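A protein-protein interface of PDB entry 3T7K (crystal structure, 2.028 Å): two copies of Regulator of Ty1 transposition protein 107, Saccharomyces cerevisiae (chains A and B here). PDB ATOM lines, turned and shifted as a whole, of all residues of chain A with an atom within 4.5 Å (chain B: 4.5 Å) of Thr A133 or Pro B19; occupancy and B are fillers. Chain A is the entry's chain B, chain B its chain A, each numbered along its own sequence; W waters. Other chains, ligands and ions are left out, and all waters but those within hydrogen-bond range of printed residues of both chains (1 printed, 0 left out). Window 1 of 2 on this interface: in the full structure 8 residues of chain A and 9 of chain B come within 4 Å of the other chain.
N of Tyr B21 sits at hydrogen-bond distance from O of Leu B46. The backbone carbonyl oxygen of Thr A133 sits at hydrogen-bond distance from the guanidinium group of Arg A138, 2.9 Å away. OE1 of Glu A137 sits at hydrogen-bond distance from N of Lys A134 (3.1 Å).
CG of Pro A132 touches CB of Pro B19 (3.9 Å). Pro A132 touches Tyr B21. CG2 of Thr A133 touches OE2 of Glu B17 (3.7 Å). Pro B19 touches Thr A133. Glu A137 touches Glu B17. Glu B17 touches Arg A138 (CB to O, 3.9 Å).
Thr A133 touches just these residues of chain B: Glu B17 (3.7 Å) and Pro B19 (3.5 Å). Pro B19 touches just these residues of chain A: Pro A132 and Thr A133. Of the printed residues of chain B, Pro A132 touches Pro B19 (3.9 Å) and Tyr B21 (3.4 Å). Printed residues of chain B within 4 Å of Arg A138: Glu B17. Printed residues of chain A within 4 Å of Glu B17: Thr A133 (3.7 Å), Glu A137 (3.2 Å) and Arg A138 (3.9 Å). Of the printed residues of chain A, Tyr B21 touches Pro A132. The nearest printed residue of chain B that does not touch Pro A132 is Ile B109 (4.4 Å).
Printed residues of chain B that touch a printed residue of chain A: Glu B17, Pro B19 and Tyr B21. Among the printed residues, 6 pairs touch across the chains. Among the printed residues, no Asp or Glu carboxylate lies within 4 Å of a Lys or Arg side-chain nitrogen of the other chain.
No position is printed for both chains. Of the 6 pairs that touch across the chains among the printed residues, none has its exchanged pair printed and touching as well.
Water W1 lies within hydrogen-bond range of O of Pro A132 (2.7 Å), OE2 of Glu A137 (2.8 Å) and N of Asn B20 (2.9 Å).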
ATOM      1  N   LEU A 131      12.392  -4.696 -34.314  1.00  0.00           N
ATOM      2  CA  LEU A 131      12.724  -4.141 -33.011  1.00  0.00           C
ATOM      3  C   LEU A 131      12.028  -4.949 -31.933  1.00  0.00           C
ATOM      4  O   LEU A 131      10.926  -5.458 -32.138  1.00  0.00           O
ATOM      5  CB  LEU A 131      12.332  -2.677 -32.926  1.00  0.00           C
ATOM      6  CG  LEU A 131      13.162  -1.782 -33.843  1.00  0.00           C
ATOM      7  CD1 LEU A 131      12.554  -0.377 -33.909  1.00  0.00           C
ATOM      8  CD2 LEU A 131      14.611  -1.737 -33.365  1.00  0.00           C
ATOM      9  N   PRO A 132      12.690  -5.095 -30.788  1.00  0.00           N
ATOM     10  CA  PRO A 132      12.194  -5.878 -29.655  1.00  0.00           C
ATOM     11  C   PRO A 132      11.110  -5.134 -28.867  1.00  0.00           C
ATOM     12  O   PRO A 132      10.644  -5.644 -27.846  1.00  0.00           O
ATOM     13  CB  PRO A 132      13.443  -6.052 -28.791  1.00  0.00           C
ATOM     14  CG  PRO A 132      14.263  -4.867 -29.113  1.00  0.00           C
ATOM     15  CD  PRO A 132      14.065  -4.622 -30.567  1.00  0.00           C
ATOM     16  N   THR A 133      10.711  -3.958 -29.350  1.00  0.00           N
ATOM     17  CA  THR A 133       9.657  -3.184 -28.708  1.00  0.00           C
ATOM     18  C   THR A 133       8.588  -2.818 -29.725  1.00  0.00           C
ATOM     19  O   THR A 133       8.828  -2.881 -30.937  1.00  0.00           O
ATOM     20  CB  THR A 133      10.213  -1.882 -28.098  1.00  0.00           C
ATOM     21  OG1 THR A 133      10.856  -1.112 -29.125  1.00  0.00           O
ATOM     22  CG2 THR A 133      11.225  -2.199 -27.019  1.00  0.00           C
ATOM     23  N   LYS A 134       7.411  -2.445 -29.231  1.00  0.00           N
ATOM     24  CA  LYS A 134       6.378  -1.862 -30.082  1.00  0.00           C
ATOM     25  C   LYS A 134       6.456  -0.332 -30.032  1.00  0.00           C
ATOM     26  O   LYS A 134       7.047   0.231 -29.130  1.00  0.00           O
ATOM     27  CB  LYS A 134       4.993  -2.331 -29.668  1.00  0.00           C
ATOM     28  CG  LYS A 134       4.826  -3.810 -29.653  1.00  0.00           C
ATOM     29  CD  LYS A 134       4.950  -4.392 -31.045  1.00  0.00           C
ATOM     30  CE  LYS A 134       4.532  -5.855 -31.009  1.00  0.00           C
ATOM     31  NZ  LYS A 134       4.894  -6.570 -32.251  1.00  0.00           N
ATOM     32  N   VAL A 135       5.856   0.321 -31.017  1.00  0.00           N
ATOM     33  CA  VAL A 135       6.096   1.729 -31.260  1.00  0.00           C
ATOM     34  C   VAL A 135       5.651   2.563 -30.042  1.00  0.00           C
ATOM     35  O   VAL A 135       6.371   3.444 -29.609  1.00  0.00           O
ATOM     36  CB  VAL A 135       5.406   2.202 -32.565  1.00  0.00           C
ATOM     37  CG1 VAL A 135       3.914   1.924 -32.512  1.00  0.00           C
ATOM     38  CG2 VAL A 135       5.676   3.688 -32.824  1.00  0.00           C
ATOM     39  N   GLU A 137       5.126   1.368 -26.991  1.00  0.00           N
ATOM     40  CA  GLU A 137       5.916   0.898 -25.885  1.00  0.00           C
ATOM     41  C   GLU A 137       7.234   1.660 -25.839  1.00  0.00           C
ATOM     42  O   GLU A 137       7.657   2.112 -24.770  1.00  0.00           O
ATOM     43  CB  GLU A 137       6.151  -0.606 -26.021  1.00  0.00           C
ATOM     44  CG  GLU A 137       7.195  -1.126 -25.096  1.00  0.00           C
ATOM     45  CD  GLU A 137       7.459  -2.597 -25.283  1.00  0.00           C
ATOM     46  OE1 GLU A 137       6.990  -3.191 -26.288  1.00  0.00           O
ATOM     47  OE2 GLU A 137       8.142  -3.151 -24.406  1.00  0.00           O
ATOM     48  N   ARG A 138       7.880   1.800 -26.997  1.00  0.00           N
ATOM     49  CA  ARG A 138       9.064   2.649 -27.138  1.00  0.00           C
ATOM     50  C   ARG A 138       8.834   4.083 -26.690  1.00  0.00           C
ATOM     51  O   ARG A 138       9.774   4.758 -26.261  1.00  0.00           O
ATOM     52  CB  ARG A 138       9.503   2.739 -28.603  1.00  0.00           C
ATOM     53  CG  ARG A 138      10.280   1.587 -29.091  1.00  0.00           C
ATOM     54  CD  ARG A 138      11.088   1.932 -30.338  1.00  0.00           C
ATOM     55  NE  ARG A 138      10.305   2.056 -31.569  1.00  0.00           N
ATOM     56  CZ  ARG A 138       9.685   1.056 -32.181  1.00  0.00           C
ATOM     57  NH1 ARG A 138       9.701  -0.171 -31.661  1.00  0.00           N
ATOM     58  NH2 ARG A 138       9.037   1.280 -33.317  1.00  0.00           N
ATOM     59  N   GLU B  17      13.762   3.973 -22.538  1.00  0.00           N
ATOM     60  CA  GLU B  17      12.862   2.843 -22.368  1.00  0.00           C
ATOM     61  C   GLU B  17      13.657   1.570 -22.652  1.00  0.00           C
ATOM     62  O   GLU B  17      14.577   1.593 -23.469  1.00  0.00           O
ATOM     63  CB  GLU B  17      11.685   2.989 -23.334  1.00  0.00           C
ATOM     64  CG  GLU B  17      10.629   1.918 -23.238  1.00  0.00           C
ATOM     65  CD  GLU B  17      10.951   0.696 -24.088  1.00  0.00           C
ATOM     66  OE1 GLU B  17      12.009   0.690 -24.783  1.00  0.00           O
ATOM     67  OE2 GLU B  17      10.136  -0.256 -24.057  1.00  0.00           O
ATOM     68  N   LEU B  18      13.322   0.474 -21.970  1.00  0.00           N
ATOM     69  CA  LEU B  18      14.064  -0.788 -22.118  1.00  0.00           C
ATOM     70  C   LEU B  18      13.188  -1.916 -22.644  1.00  0.00           C
ATOM     71  O   LEU B  18      12.094  -2.141 -22.135  1.00  0.00           O
ATOM     72  CB  LEU B  18      14.647  -1.209 -20.771  1.00  0.00           C
ATOM     73  CG  LEU B  18      15.502  -0.153 -20.073  1.00  0.00           C
ATOM     74  CD1 LEU B  18      15.818  -0.582 -18.648  1.00  0.00           C
ATOM     75  CD2 LEU B  18      16.775   0.117 -20.873  1.00  0.00           C
ATOM     76  N   PRO B  19      13.674  -2.657 -23.652  1.00  0.00           N
ATOM     77  CA  PRO B  19      12.836  -3.754 -24.130  1.00  0.00           C
ATOM     78  C   PRO B  19      12.744  -4.852 -23.084  1.00  0.00           C
ATOM     79  O   PRO B  19      13.588  -4.927 -22.194  1.00  0.00           O
ATOM     80  CB  PRO B  19      13.585  -4.253 -25.370  1.00  0.00           C
ATOM     81  CG  PRO B  19      14.989  -3.878 -25.140  1.00  0.00           C
ATOM     82  CD  PRO B  19      14.951  -2.579 -24.377  1.00  0.00           C
ATOM     83  N   ASN B  20      11.714  -5.679 -23.186  1.00  0.00           N
ATOM     84  CA  ASN B  20      11.570  -6.847 -22.334  1.00  0.00           C
ATOM     85  C   ASN B  20      11.640  -8.073 -23.232  1.00  0.00           C
ATOM     86  O   ASN B  20      10.659  -8.420 -23.893  1.00  0.00           O
ATOM     87  CB  ASN B  20      10.247  -6.812 -21.567  1.00  0.00           C
ATOM     88  CG  ASN B  20       9.924  -8.145 -20.889  1.00  0.00           C
ATOM     89  OD1 ASN B  20      10.817  -8.896 -20.499  1.00  0.00           O
ATOM     90  ND2 ASN B  20       8.646  -8.446 -20.767  1.00  0.00           N
ATOM     91  N   TYR B  21      12.807  -8.699 -23.287  1.00  0.00           N
ATOM     92  CA  TYR B  21      13.026  -9.814 -24.227  1.00  0.00           C
ATOM     93  C   TYR B  21      12.310 -11.092 -23.817  1.00  0.00           C
ATOM     94  O   TYR B  21      12.182 -12.024 -24.625  1.00  0.00           O
ATOM     95  CB  TYR B  21      14.525 -10.079 -24.425  1.00  0.00           C
ATOM     96  CG  TYR B  21      15.235  -9.015 -25.206  1.00  0.00           C
ATOM     97  CD1 TYR B  21      15.152  -8.967 -26.584  1.00  0.00           C
ATOM     98  CD2 TYR B  21      15.982  -8.042 -24.560  1.00  0.00           C
ATOM     99  CE1 TYR B  21      15.798  -7.971 -27.305  1.00  0.00           C
ATOM    100  CE2 TYR B  21      16.630  -7.058 -25.263  1.00  0.00           C
ATOM    101  CZ  TYR B  21      16.531  -7.014 -26.625  1.00  0.00           C
ATOM    102  OH  TYR B  21      17.195  -6.024 -27.310  1.00  0.00           O
ATOM    103  N   GLN B  45      17.084  -6.783 -16.077  1.00  0.00           N
ATOM    104  CA  GLN B  45      16.292  -5.579 -16.289  1.00  0.00           C
ATOM    105  C   GLN B  45      15.720  -5.561 -17.698  1.00  0.00           C
ATOM    106  O   GLN B  45      14.794  -4.805 -17.985  1.00  0.00           O
ATOM    107  CB  GLN B  45      17.138  -4.337 -16.043  1.00  0.00           C
ATOM    108  CG  GLN B  45      17.287  -3.985 -14.569  1.00  0.00           C
ATOM    109  CD  GLN B  45      16.006  -3.431 -13.989  1.00  0.00           C
ATOM    110  OE1 GLN B  45      15.314  -4.101 -13.219  1.00  0.00           O
ATOM    111  NE2 GLN B  45      15.675  -2.201 -14.363  1.00  0.00           N
ATOM    112  N   LEU B  46      16.284  -6.390 -18.573  1.00  0.00           N
ATOM    113  CA  LEU B  46      15.847  -6.450 -19.962  1.00  0.00           C
ATOM    114  C   LEU B  46      14.985  -7.669 -20.200  1.00  0.00           C
ATOM    115  O   LEU B  46      14.709  -8.030 -21.336  1.00  0.00           O
ATOM    116  CB  LEU B  46      17.047  -6.464 -20.910  1.00  0.00           C
ATOM    117  CG  LEU B  46      17.865  -5.168 -20.918  1.00  0.00           C
ATOM    118  CD1 LEU B  46      19.107  -5.308 -21.778  1.00  0.00           C
ATOM    119  CD2 LEU B  46      17.019  -3.999 -21.397  1.00  0.00           C
ATOM    120  N   ILE B 109      18.093   0.901 -27.470  1.00  0.00           N
ATOM    121  CA  ILE B 109      18.468  -0.508 -27.618  1.00  0.00           C
ATOM    122  C   ILE B 109      17.689  -1.125 -28.769  1.00  0.00           C
ATOM    123  O   ILE B 109      16.469  -1.110 -28.773  1.00  0.00           O
ATOM    124  CB  ILE B 109      18.163  -1.283 -26.329  1.00  0.00           C
ATOM    125  CG1 ILE B 109      18.951  -0.683 -25.165  1.00  0.00           C
ATOM    126  CG2 ILE B 109      18.483  -2.760 -26.497  1.00  0.00           C
ATOM    127  CD1 ILE B 109      18.531  -1.202 -23.803  1.00  0.00           C
HETATM  128  O   HOH W   1       9.763  -5.299 -25.303  1.00  0.00           O
